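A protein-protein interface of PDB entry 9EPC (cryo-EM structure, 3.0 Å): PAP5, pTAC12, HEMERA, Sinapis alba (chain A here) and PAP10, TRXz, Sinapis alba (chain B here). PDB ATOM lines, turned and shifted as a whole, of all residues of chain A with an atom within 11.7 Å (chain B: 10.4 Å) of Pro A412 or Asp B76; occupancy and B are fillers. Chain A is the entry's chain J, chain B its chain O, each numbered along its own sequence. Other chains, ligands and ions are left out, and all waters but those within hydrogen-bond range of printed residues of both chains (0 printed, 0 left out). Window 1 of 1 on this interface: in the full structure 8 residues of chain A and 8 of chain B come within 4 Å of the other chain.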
ATOM      1  N   MET A 402     -17.738   8.448  22.794  1.00  0.00           N
ATOM      2  CA  MET A 402     -18.073   7.310  21.940  1.00  0.00           C
ATOM      3  C   MET A 402     -17.054   6.181  22.113  1.00  0.00           C
ATOM      4  O   MET A 402     -16.257   5.878  21.227  1.00  0.00           O
ATOM      5  CB  MET A 402     -18.176   7.739  20.473  1.00  0.00           C
ATOM      6  CG  MET A 402     -19.266   7.036  19.700  1.00  0.00           C
ATOM      7  SD  MET A 402     -20.898   7.445  20.335  1.00  0.00           S
ATOM      8  CE  MET A 402     -20.836   9.230  20.268  1.00  0.00           C
ATOM      9  N   ASP A 403     -17.079   5.604  23.312  1.00  0.00           N
ATOM     10  CA  ASP A 403     -16.197   4.494  23.650  1.00  0.00           C
ATOM     11  C   ASP A 403     -16.223   3.427  22.567  1.00  0.00           C
ATOM     12  O   ASP A 403     -17.257   2.802  22.318  1.00  0.00           O
ATOM     13  CB  ASP A 403     -16.613   3.892  24.992  1.00  0.00           C
ATOM     14  CG  ASP A 403     -15.767   2.702  25.379  1.00  0.00           C
ATOM     15  OD1 ASP A 403     -14.597   2.902  25.763  1.00  0.00           O
ATOM     16  OD2 ASP A 403     -16.268   1.564  25.299  1.00  0.00           O
ATOM     17  N   PHE A 404     -15.075   3.220  21.929  1.00  0.00           N
ATOM     18  CA  PHE A 404     -14.953   2.284  20.822  1.00  0.00           C
ATOM     19  C   PHE A 404     -14.758   0.848  21.278  1.00  0.00           C
ATOM     20  O   PHE A 404     -14.607  -0.038  20.431  1.00  0.00           O
ATOM     21  CB  PHE A 404     -13.797   2.697  19.912  1.00  0.00           C
ATOM     22  CG  PHE A 404     -14.053   3.960  19.147  1.00  0.00           C
ATOM     23  CD1 PHE A 404     -15.313   4.241  18.655  1.00  0.00           C
ATOM     24  CD2 PHE A 404     -13.036   4.867  18.923  1.00  0.00           C
ATOM     25  CE1 PHE A 404     -15.550   5.400  17.953  1.00  0.00           C
ATOM     26  CE2 PHE A 404     -13.270   6.027  18.220  1.00  0.00           C
ATOM     27  CZ  PHE A 404     -14.528   6.293  17.735  1.00  0.00           C
ATOM     28  N   ARG A 405     -14.742   0.597  22.585  1.00  0.00           N
ATOM     29  CA  ARG A 405     -14.645  -0.751  23.121  1.00  0.00           C
ATOM     30  C   ARG A 405     -15.993  -1.284  23.587  1.00  0.00           C
ATOM     31  O   ARG A 405     -16.039  -2.216  24.394  1.00  0.00           O
ATOM     32  CB  ARG A 405     -13.633  -0.788  24.264  1.00  0.00           C
ATOM     33  CG  ARG A 405     -12.224  -0.452  23.834  1.00  0.00           C
ATOM     34  CD  ARG A 405     -11.788  -1.340  22.688  1.00  0.00           C
ATOM     35  NE  ARG A 405     -11.898  -2.751  23.029  1.00  0.00           N
ATOM     36  CZ  ARG A 405     -10.943  -3.454  23.619  1.00  0.00           C
ATOM     37  NH1 ARG A 405      -9.785  -2.908  23.947  1.00  0.00           N
ATOM     38  NH2 ARG A 405     -11.155  -4.738  23.889  1.00  0.00           N
ATOM     39  N   GLY A 406     -17.082  -0.712  23.097  1.00  0.00           N
ATOM     40  CA  GLY A 406     -18.403  -1.151  23.478  1.00  0.00           C
ATOM     41  C   GLY A 406     -18.779  -2.452  22.814  1.00  0.00           C
ATOM     42  O   GLY A 406     -18.081  -2.976  21.934  1.00  0.00           O
ATOM     43  N   PRO A 407     -19.912  -3.010  23.246  1.00  0.00           N
ATOM     44  CA  PRO A 407     -20.370  -4.282  22.669  1.00  0.00           C
ATOM     45  C   PRO A 407     -20.728  -4.192  21.199  1.00  0.00           C
ATOM     46  O   PRO A 407     -20.747  -5.226  20.523  1.00  0.00           O
ATOM     47  CB  PRO A 407     -21.604  -4.629  23.515  1.00  0.00           C
ATOM     48  CG  PRO A 407     -21.498  -3.775  24.735  1.00  0.00           C
ATOM     49  CD  PRO A 407     -20.819  -2.526  24.296  1.00  0.00           C
ATOM     50  N   ASP A 408     -21.021  -3.004  20.683  1.00  0.00           N
ATOM     51  CA  ASP A 408     -21.449  -2.847  19.302  1.00  0.00           C
ATOM     52  C   ASP A 408     -20.302  -2.559  18.346  1.00  0.00           C
ATOM     53  O   ASP A 408     -20.546  -2.369  17.151  1.00  0.00           O
ATOM     54  CB  ASP A 408     -22.491  -1.731  19.197  1.00  0.00           C
ATOM     55  CG  ASP A 408     -23.806  -2.104  19.843  1.00  0.00           C
ATOM     56  OD1 ASP A 408     -24.115  -3.312  19.907  1.00  0.00           O
ATOM     57  OD2 ASP A 408     -24.534  -1.191  20.283  1.00  0.00           O
ATOM     58  N   PHE A 409     -19.068  -2.528  18.832  1.00  0.00           N
ATOM     59  CA  PHE A 409     -17.909  -2.230  18.006  1.00  0.00           C
ATOM     60  C   PHE A 409     -17.064  -3.480  17.817  1.00  0.00           C
ATOM     61  O   PHE A 409     -16.933  -4.298  18.732  1.00  0.00           O
ATOM     62  CB  PHE A 409     -17.060  -1.124  18.625  1.00  0.00           C
ATOM     63  CG  PHE A 409     -17.724   0.217  18.633  1.00  0.00           C
ATOM     64  CD1 PHE A 409     -17.593   1.072  17.557  1.00  0.00           C
ATOM     65  CD2 PHE A 409     -18.478   0.622  19.716  1.00  0.00           C
ATOM     66  CE1 PHE A 409     -18.200   2.305  17.562  1.00  0.00           C
ATOM     67  CE2 PHE A 409     -19.088   1.855  19.724  1.00  0.00           C
ATOM     68  CZ  PHE A 409     -18.949   2.696  18.646  1.00  0.00           C
ATOM     69  N   HIS A 410     -16.491  -3.616  16.626  1.00  0.00           N
ATOM     70  CA  HIS A 410     -15.597  -4.723  16.337  1.00  0.00           C
ATOM     71  C   HIS A 410     -14.309  -4.577  17.143  1.00  0.00           C
ATOM     72  O   HIS A 410     -14.085  -3.589  17.846  1.00  0.00           O
ATOM     73  CB  HIS A 410     -15.298  -4.777  14.843  1.00  0.00           C
ATOM     74  CG  HIS A 410     -14.697  -3.518  14.306  1.00  0.00           C
ATOM     75  ND1 HIS A 410     -13.377  -3.177  14.510  1.00  0.00           N
ATOM     76  CD2 HIS A 410     -15.237  -2.510  13.582  1.00  0.00           C
ATOM     77  CE1 HIS A 410     -13.129  -2.017  13.930  1.00  0.00           C
ATOM     78  NE2 HIS A 410     -14.242  -1.591  13.360  1.00  0.00           N
ATOM     79  N   GLU A 411     -13.447  -5.580  17.034  1.00  0.00           N
ATOM     80  CA  GLU A 411     -12.172  -5.532  17.723  1.00  0.00           C
ATOM     81  C   GLU A 411     -11.299  -4.425  17.139  1.00  0.00           C
ATOM     82  O   GLU A 411     -11.443  -4.062  15.969  1.00  0.00           O
ATOM     83  CB  GLU A 411     -11.457  -6.874  17.611  1.00  0.00           C
ATOM     84  CG  GLU A 411     -12.148  -8.005  18.348  1.00  0.00           C
ATOM     85  CD  GLU A 411     -12.240  -7.757  19.839  1.00  0.00           C
ATOM     86  OE1 GLU A 411     -13.186  -7.070  20.276  1.00  0.00           O
ATOM     87  OE2 GLU A 411     -11.359  -8.244  20.576  1.00  0.00           O
ATOM     88  N   PRO A 412     -10.404  -3.852  17.943  1.00  0.00           N
ATOM     89  CA  PRO A 412      -9.520  -2.803  17.427  1.00  0.00           C
ATOM     90  C   PRO A 412      -8.690  -3.307  16.257  1.00  0.00           C
ATOM     91  O   PRO A 412      -8.160  -4.419  16.278  1.00  0.00           O
ATOM     92  CB  PRO A 412      -8.639  -2.458  18.632  1.00  0.00           C
ATOM     93  CG  PRO A 412      -9.441  -2.865  19.812  1.00  0.00           C
ATOM     94  CD  PRO A 412     -10.221  -4.069  19.387  1.00  0.00           C
ATOM     95  N   THR A 413      -8.576  -2.472  15.233  1.00  0.00           N
ATOM     96  CA  THR A 413      -7.853  -2.855  14.030  1.00  0.00           C
ATOM     97  C   THR A 413      -6.355  -2.747  14.276  1.00  0.00           C
ATOM     98  O   THR A 413      -5.866  -1.655  14.587  1.00  0.00           O
ATOM     99  CB  THR A 413      -8.252  -1.969  12.860  1.00  0.00           C
ATOM    100  OG1 THR A 413      -9.667  -2.052  12.660  1.00  0.00           O
ATOM    101  CG2 THR A 413      -7.545  -2.419  11.596  1.00  0.00           C
ATOM    102  N   PRO A 414      -5.599  -3.834  14.157  1.00  0.00           N
ATOM    103  CA  PRO A 414      -4.152  -3.746  14.366  1.00  0.00           C
ATOM    104  C   PRO A 414      -3.480  -2.959  13.257  1.00  0.00           C
ATOM    105  O   PRO A 414      -3.951  -2.916  12.118  1.00  0.00           O
ATOM    106  CB  PRO A 414      -3.698  -5.212  14.353  1.00  0.00           C
ATOM    107  CG  PRO A 414      -4.949  -6.021  14.491  1.00  0.00           C
ATOM    108  CD  PRO A 414      -6.029  -5.208  13.865  1.00  0.00           C
ATOM    109  N   ASN A 415      -2.366  -2.322  13.607  1.00  0.00           N
ATOM    110  CA  ASN A 415      -1.523  -1.703  12.597  1.00  0.00           C
ATOM    111  C   ASN A 415      -1.028  -2.769  11.633  1.00  0.00           C
ATOM    112  O   ASN A 415      -0.606  -3.850  12.053  1.00  0.00           O
ATOM    113  CB  ASN A 415      -0.346  -0.987  13.256  1.00  0.00           C
ATOM    114  CG  ASN A 415       0.621  -0.410  12.248  1.00  0.00           C
ATOM    115  OD1 ASN A 415       1.604  -1.049  11.877  1.00  0.00           O
ATOM    116  ND2 ASN A 415       0.345   0.805  11.793  1.00  0.00           N
ATOM    117  N   MET A 416      -1.095  -2.472  10.333  1.00  0.00           N
ATOM    118  CA  MET A 416      -0.788  -3.494   9.340  1.00  0.00           C
ATOM    119  C   MET A 416       0.646  -3.985   9.473  1.00  0.00           C
ATOM    120  O   MET A 416       0.901  -5.193   9.410  1.00  0.00           O
ATOM    121  CB  MET A 416      -1.043  -2.968   7.931  1.00  0.00           C
ATOM    122  CG  MET A 416      -1.151  -4.078   6.903  1.00  0.00           C
ATOM    123  SD  MET A 416      -2.608  -5.097   7.176  1.00  0.00           S
ATOM    124  CE  MET A 416      -2.016  -6.694   6.635  1.00  0.00           C
ATOM    125  N   SER A 418       2.201  -4.366  12.090  1.00  0.00           N
ATOM    126  CA  SER A 418       2.388  -5.058  13.357  1.00  0.00           C
ATOM    127  C   SER A 418       1.672  -6.395  13.400  1.00  0.00           C
ATOM    128  O   SER A 418       2.096  -7.281  14.148  1.00  0.00           O
ATOM    129  CB  SER A 418       1.906  -4.191  14.524  1.00  0.00           C
ATOM    130  OG  SER A 418       2.589  -2.951  14.548  1.00  0.00           O
ATOM    131  N   TYR A 419       0.610  -6.573  12.615  1.00  0.00           N
ATOM    132  CA  TYR A 419      -0.003  -7.882  12.451  1.00  0.00           C
ATOM    133  C   TYR A 419       0.900  -8.797  11.636  1.00  0.00           C
ATOM    134  O   TYR A 419       1.018  -9.991  11.934  1.00  0.00           O
ATOM    135  CB  TYR A 419      -1.367  -7.716  11.784  1.00  0.00           C
ATOM    136  CG  TYR A 419      -2.276  -8.912  11.876  1.00  0.00           C
ATOM    137  CD1 TYR A 419      -2.403  -9.623  13.057  1.00  0.00           C
ATOM    138  CD2 TYR A 419      -3.035  -9.311  10.785  1.00  0.00           C
ATOM    139  CE1 TYR A 419      -3.242 -10.713  13.145  1.00  0.00           C
ATOM    140  CE2 TYR A 419      -3.879 -10.396  10.863  1.00  0.00           C
ATOM    141  CZ  TYR A 419      -3.979 -11.094  12.045  1.00  0.00           C
ATOM    142  OH  TYR A 419      -4.821 -12.179  12.125  1.00  0.00           O
ATOM    143  N   GLU A 422       3.742  -9.686  13.944  1.00  0.00           N
ATOM    144  CA  GLU A 422       3.298 -10.638  14.955  1.00  0.00           C
ATOM    145  C   GLU A 422       3.219 -12.047  14.386  1.00  0.00           C
ATOM    146  O   GLU A 422       3.618 -13.015  15.043  1.00  0.00           O
ATOM    147  CB  GLU A 422       1.945 -10.211  15.519  1.00  0.00           C
ATOM    148  CG  GLU A 422       1.467 -11.066  16.675  1.00  0.00           C
ATOM    149  CD  GLU A 422       2.274 -10.838  17.936  1.00  0.00           C
ATOM    150  OE1 GLU A 422       2.881  -9.755  18.068  1.00  0.00           O
ATOM    151  OE2 GLU A 422       2.304 -11.742  18.797  1.00  0.00           O
ATOM    152  N   GLY B  70       0.953  -9.848  22.531  1.00  0.00           N
ATOM    153  CA  GLY B  70       1.964  -9.971  21.498  1.00  0.00           C
ATOM    154  C   GLY B  70       3.078  -8.950  21.627  1.00  0.00           C
ATOM    155  O   GLY B  70       2.890  -7.889  22.221  1.00  0.00           O
ATOM    156  N   PHE B  72       4.454  -7.208  19.179  1.00  0.00           N
ATOM    157  CA  PHE B  72       4.204  -6.066  18.311  1.00  0.00           C
ATOM    158  C   PHE B  72       2.795  -5.513  18.427  1.00  0.00           C
ATOM    159  O   PHE B  72       2.609  -4.298  18.311  1.00  0.00           O
ATOM    160  CB  PHE B  72       4.481  -6.446  16.854  1.00  0.00           C
ATOM    161  CG  PHE B  72       5.803  -7.122  16.654  1.00  0.00           C
ATOM    162  CD1 PHE B  72       6.971  -6.383  16.597  1.00  0.00           C
ATOM    163  CD2 PHE B  72       5.879  -8.497  16.532  1.00  0.00           C
ATOM    164  CE1 PHE B  72       8.189  -7.003  16.419  1.00  0.00           C
ATOM    165  CE2 PHE B  72       7.094  -9.123  16.354  1.00  0.00           C
ATOM    166  CZ  PHE B  72       8.251  -8.374  16.297  1.00  0.00           C
ATOM    167  N   VAL B  73       1.798  -6.364  18.651  1.00  0.00           N
ATOM    168  CA  VAL B  73       0.418  -5.931  18.828  1.00  0.00           C
ATOM    169  C   VAL B  73       0.043  -6.133  20.288  1.00  0.00           C
ATOM    170  O   VAL B  73       0.192  -7.235  20.832  1.00  0.00           O
ATOM    171  CB  VAL B  73      -0.545  -6.681  17.896  1.00  0.00           C
ATOM    172  CG1 VAL B  73      -0.507  -6.077  16.506  1.00  0.00           C
ATOM    173  CG2 VAL B  73      -0.194  -8.151  17.842  1.00  0.00           C
ATOM    174  N   ARG B  74      -0.426  -5.066  20.924  1.00  0.00           N
ATOM    175  CA  ARG B  74      -0.861  -5.143  22.310  1.00  0.00           C
ATOM    176  C   ARG B  74      -2.115  -6.000  22.425  1.00  0.00           C
ATOM    177  O   ARG B  74      -2.998  -5.953  21.565  1.00  0.00           O
ATOM    178  CB  ARG B  74      -1.124  -3.737  22.846  1.00  0.00           C
ATOM    179  CG  ARG B  74      -1.535  -3.683  24.300  1.00  0.00           C
ATOM    180  CD  ARG B  74      -0.455  -4.254  25.191  1.00  0.00           C
ATOM    181  NE  ARG B  74      -0.837  -4.213  26.596  1.00  0.00           N
ATOM    182  CZ  ARG B  74      -0.182  -4.834  27.566  1.00  0.00           C
ATOM    183  NH1 ARG B  74       0.890  -5.565  27.316  1.00  0.00           N
ATOM    184  NH2 ARG B  74      -0.618  -4.722  28.817  1.00  0.00           N
ATOM    185  N   GLU B  75      -2.183  -6.801  23.485  1.00  0.00           N
ATOM    186  CA  GLU B  75      -3.374  -7.599  23.731  1.00  0.00           C
ATOM    187  C   GLU B  75      -4.560  -6.688  24.016  1.00  0.00           C
ATOM    188  O   GLU B  75      -4.439  -5.690  24.731  1.00  0.00           O
ATOM    189  CB  GLU B  75      -3.157  -8.552  24.908  1.00  0.00           C
ATOM    190  CG  GLU B  75      -1.833  -9.301  24.897  1.00  0.00           C
ATOM    191  CD  GLU B  75      -0.736  -8.556  25.630  1.00  0.00           C
ATOM    192  OE1 GLU B  75      -0.755  -7.310  25.619  1.00  0.00           O
ATOM    193  OE2 GLU B  75       0.140  -9.215  26.226  1.00  0.00           O
ATOM    194  N   ASP B  76      -5.716  -7.037  23.452  1.00  0.00           N
ATOM    195  CA  ASP B  76      -6.897  -6.202  23.618  1.00  0.00           C
ATOM    196  C   ASP B  76      -7.477  -6.283  25.021  1.00  0.00           C
ATOM    197  O   ASP B  76      -8.134  -5.335  25.460  1.00  0.00           O
ATOM    198  CB  ASP B  76      -7.964  -6.596  22.600  1.00  0.00           C
ATOM    199  CG  ASP B  76      -7.413  -6.708  21.197  1.00  0.00           C
ATOM    200  OD1 ASP B  76      -6.656  -7.663  20.929  1.00  0.00           O
ATOM    201  OD2 ASP B  76      -7.736  -5.840  20.361  1.00  0.00           O
ATOM    202  N   TYR B  77      -7.249  -7.383  25.731  1.00  0.00           N
ATOM    203  CA  TYR B  77      -7.876  -7.620  27.023  1.00  0.00           C
ATOM    204  C   TYR B  77      -6.811  -7.927  28.061  1.00  0.00           C
ATOM    205  O   TYR B  77      -5.910  -8.735  27.812  1.00  0.00           O
ATOM    206  CB  TYR B  77      -8.884  -8.765  26.930  1.00  0.00           C
ATOM    207  CG  TYR B  77      -9.919  -8.541  25.858  1.00  0.00           C
ATOM    208  CD1 TYR B  77     -11.080  -7.835  26.128  1.00  0.00           C
ATOM    209  CD2 TYR B  77      -9.728  -9.019  24.571  1.00  0.00           C
ATOM    210  CE1 TYR B  77     -12.026  -7.620  25.153  1.00  0.00           C
ATOM    211  CE2 TYR B  77     -10.669  -8.807  23.588  1.00  0.00           C
ATOM    212  CZ  TYR B  77     -11.816  -8.106  23.885  1.00  0.00           C
ATOM    213  OH  TYR B  77     -12.760  -7.892  22.910  1.00  0.00           O
ATOM    214  N   LEU B  78      -6.919  -7.284  29.222  1.00  0.00           N
ATOM    215  CA  LEU B  78      -5.966  -7.479  30.302  1.00  0.00           C
ATOM    216  C   LEU B  78      -6.470  -8.415  31.390  1.00  0.00           C
ATOM    217  O   LEU B  78      -5.651  -8.997  32.109  1.00  0.00           O
ATOM    218  CB  LEU B  78      -5.601  -6.133  30.935  1.00  0.00           C
ATOM    219  CG  LEU B  78      -5.058  -5.074  29.978  1.00  0.00           C
ATOM    220  CD1 LEU B  78      -4.639  -3.836  30.744  1.00  0.00           C
ATOM    221  CD2 LEU B  78      -3.899  -5.629  29.173  1.00  0.00           C
ATOM    222  N   VAL B  79      -7.783  -8.572  31.530  1.00  0.00           N
ATOM    223  CA  VAL B  79      -8.348  -9.443  32.555  1.00  0.00           C
ATOM    224  C   VAL B  79      -8.203 -10.884  32.080  1.00  0.00           C
ATOM    225  O   VAL B  79      -8.836 -11.294  31.105  1.00  0.00           O
ATOM    226  CB  VAL B  79      -9.811  -9.096  32.843  1.00  0.00           C
ATOM    227  CG1 VAL B  79     -10.375 -10.030  33.893  1.00  0.00           C
ATOM    228  CG2 VAL B  79      -9.927  -7.654  33.299  1.00  0.00           C
ATOM    229  N   ARG B  80      -7.372 -11.655  32.772  1.00  0.00           N
ATOM    230  CA  ARG B  80      -7.054 -13.017  32.371  1.00  0.00           C
ATOM    231  C   ARG B  80      -8.064 -13.992  32.961  1.00  0.00           C
ATOM    232  O   ARG B  80      -8.387 -13.917  34.150  1.00  0.00           O
ATOM    233  CB  ARG B  80      -5.640 -13.384  32.820  1.00  0.00           C
ATOM    234  CG  ARG B  80      -5.252 -14.826  32.557  1.00  0.00           C
ATOM    235  CD  ARG B  80      -3.844 -15.125  33.051  1.00  0.00           C
ATOM    236  NE  ARG B  80      -3.726 -15.012  34.501  1.00  0.00           N
ATOM    237  CZ  ARG B  80      -3.257 -13.948  35.136  1.00  0.00           C
ATOM    238  NH1 ARG B  80      -2.848 -12.874  34.479  1.00  0.00           N
ATOM    239  NH2 ARG B  80      -3.193 -13.960  36.464  1.00  0.00           N
ATOM    240  N   ALA B 115     -17.981  -6.633  32.390  1.00  0.00           N
ATOM    241  CA  ALA B 115     -16.687  -7.011  31.832  1.00  0.00           C
ATOM    242  C   ALA B 115     -15.912  -5.804  31.328  1.00  0.00           C
ATOM    243  O   ALA B 115     -14.679  -5.783  31.405  1.00  0.00           O
ATOM    244  CB  ALA B 115     -16.873  -8.027  30.707  1.00  0.00           C
ATOM    245  N   GLN B 116     -16.609  -4.791  30.814  1.00  0.00           N
ATOM    246  CA  GLN B 116     -15.922  -3.594  30.349  1.00  0.00           C
ATOM    247  C   GLN B 116     -15.285  -2.827  31.499  1.00  0.00           C
ATOM    248  O   GLN B 116     -14.216  -2.232  31.326  1.00  0.00           O
ATOM    249  CB  GLN B 116     -16.893  -2.696  29.589  1.00  0.00           C
ATOM    250  CG  GLN B 116     -17.626  -3.397  28.471  1.00  0.00           C
ATOM    251  CD  GLN B 116     -18.609  -2.490  27.773  1.00  0.00           C
ATOM    252  OE1 GLN B 116     -19.634  -2.941  27.267  1.00  0.00           O
ATOM    253  NE2 GLN B 116     -18.302  -1.201  27.738  1.00  0.00           N
ATOM    254  N   LEU B 118     -14.035  -4.015  34.358  1.00  0.00           N
ATOM    255  CA  LEU B 118     -12.813  -4.665  34.820  1.00  0.00           C
ATOM    256  C   LEU B 118     -11.642  -4.346  33.904  1.00  0.00           C
ATOM    257  O   LEU B 118     -10.525  -4.109  34.375  1.00  0.00           O
ATOM    258  CB  LEU B 118     -13.015  -6.174  34.927  1.00  0.00           C
ATOM    259  CG  LEU B 118     -13.735  -6.670  36.180  1.00  0.00           C
ATOM    260  CD1 LEU B 118     -13.314  -5.875  37.400  1.00  0.00           C
ATOM    261  CD2 LEU B 118     -15.220  -6.598  35.999  1.00  0.00           C
ATOM    262  N   GLU B 119     -11.876  -4.334  32.591  1.00  0.00           N
ATOM    263  CA  GLU B 119     -10.829  -3.923  31.666  1.00  0.00           C
ATOM    264  C   GLU B 119     -10.394  -2.493  31.949  1.00  0.00           C
ATOM    265  O   GLU B 119      -9.195  -2.193  31.975  1.00  0.00           O
ATOM    266  CB  GLU B 119     -11.317  -4.052  30.224  1.00  0.00           C
ATOM    267  CG  GLU B 119     -11.912  -5.403  29.877  1.00  0.00           C
ATOM    268  CD  GLU B 119     -10.862  -6.440  29.548  1.00  0.00           C
ATOM    269  OE1 GLU B 119      -9.695  -6.057  29.335  1.00  0.00           O
ATOM    270  OE2 GLU B 119     -11.207  -7.638  29.498  1.00  0.00           O
ATOM    271  N   MET B 120     -11.358  -1.599  32.176  1.00  0.00           N
ATOM    272  CA  MET B 120     -11.023  -0.231  32.554  1.00  0.00           C
ATOM    273  C   MET B 120     -10.321  -0.194  33.903  1.00  0.00           C
ATOM    274  O   MET B 120      -9.357   0.557  34.090  1.00  0.00           O
ATOM    275  CB  MET B 120     -12.287   0.626  32.581  1.00  0.00           C
ATOM    276  CG  MET B 120     -12.037   2.123  32.660  1.00  0.00           C
ATOM    277  SD  MET B 120     -11.372   2.823  31.136  1.00  0.00           S
ATOM    278  CE  MET B 120      -9.623   2.882  31.508  1.00  0.00           C
ATOM    279  N   ALA B 122      -8.545  -2.634  35.215  1.00  0.00           N
ATOM    280  CA  ALA B 122      -7.220  -3.219  35.057  1.00  0.00           C
ATOM    281  C   ALA B 122      -6.221  -2.210  34.511  1.00  0.00           C
ATOM    282  O   ALA B 122      -5.027  -2.292  34.819  1.00  0.00           O
ATOM    283  CB  ALA B 122      -7.289  -4.443  34.145  1.00  0.00           C
ATOM    284  N   VAL B 123      -6.682  -1.263  33.695  1.00  0.00           N
ATOM    285  CA  VAL B 123      -5.796  -0.205  33.222  1.00  0.00           C
ATOM    286  C   VAL B 123      -5.406   0.715  34.371  1.00  0.00           C
ATOM    287  O   VAL B 123      -4.253   1.149  34.472  1.00  0.00           O
ATOM    288  CB  VAL B 123      -6.457   0.573  32.071  1.00  0.00           C
ATOM    289  CG1 VAL B 123      -5.545   1.691  31.599  1.00  0.00           C
ATOM    290  CG2 VAL B 123      -6.780  -0.362  30.924  1.00  0.00           C
ATOM    291  N   LYS B 133     -10.754 -13.345  36.010  1.00  0.00           N
ATOM    292  CA  LYS B 133     -12.160 -13.690  35.877  1.00  0.00           C
ATOM    293  C   LYS B 133     -12.313 -15.195  35.735  1.00  0.00           C
ATOM    294  O   LYS B 133     -11.450 -15.876  35.177  1.00  0.00           O
ATOM    295  CB  LYS B 133     -12.804 -12.981  34.682  1.00  0.00           C
ATOM    296  CG  LYS B 133     -12.130 -13.257  33.356  1.00  0.00           C
ATOM    297  CD  LYS B 133     -12.754 -12.428  32.251  1.00  0.00           C
ATOM    298  CE  LYS B 133     -12.018 -12.623  30.941  1.00  0.00           C
ATOM    299  NZ  LYS B 133     -12.549 -11.738  29.871  1.00  0.00           N
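The backbone NH of Phe B72 sits at hydrogen-bond distance from the side-chain carboxylate of Glu A422, 3.2 Å away. OH of Tyr B77 is in hydrogen-bond range of OE2 of Glu A411 (2.7 Å). The backbone carbonyl oxygen of Asp B76 sits at hydrogen-bond distance from the guanidinium group of Arg A405 (3.3 Å).
The side-chain carboxylate (OD2) of Asp A403 sits close to the backbone NH (N) of Arg A405. The side-chain amide oxygen of Asn A415 sits at hydrogen-bond distance from the backbone NH of Ser A418, 3.4 Å away.
Among the printed residues, merely in contact across the chains: Pro A412 with Asp B76 (3.2 Å), Pro A407 with Gln B116 (3.2 Å), Glu A422 with Gly B70 (3.2 Å), Arg A405 with Tyr B77 (3.3 Å), Glu A422 with Val B73 (3.5 Å), Ser A418 with Val B73 (3.6 Å), Ser A418 with Phe B72 (3.7 Å) and Pro A414 with Val B73 (3.9 Å).
Of chain B, only Tyr B77 (2.7 Å) comes within 4 Å of Glu A411. Pro A412 touches just one residue of chain B: Asp B76. No residue of chain B comes within 4 Å of Thr A413. Of the printed residues of chain A, Gly B70 touches Glu A422 (3.2 Å). No residue of chain A comes within 4 Å of Glu B75. Asp B76 touches just these residues of chain A: Arg A405 and Pro A412. Tyr B77 touches just these residues of chain A: Arg A405 (3.3 Å) and Glu A411 (2.7 Å). Leu B78 touches none of the printed residues of chain A. Of the printed residues of chain A, Gln B116 touches Pro A407 (3.2 Å). Val B123 touches none of the printed residues of chain A. The nearest residue of chain B that does not touch Pro A412 is Tyr B77 (5.8 Å).
Of the 18 printed residues of chain A, 7 touch a printed residue of chain B. Hydrophobic or aromatic side chains of chain A that line the printed part of chain B: Pro A407, Pro A412 and Pro A414. Of the 18 printed residues of chain B, 6 touch a printed residue of chain A. Printed residues of chain B that touch a printed residue of chain A: Gly B70, Phe B72, Val B73, Asp B76, Tyr B77 and Gln B116. Among the printed residues, no Asp or Glu carboxylate lies within 4 Å of a Lys or Arg side-chain nitrogen of the other chain.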
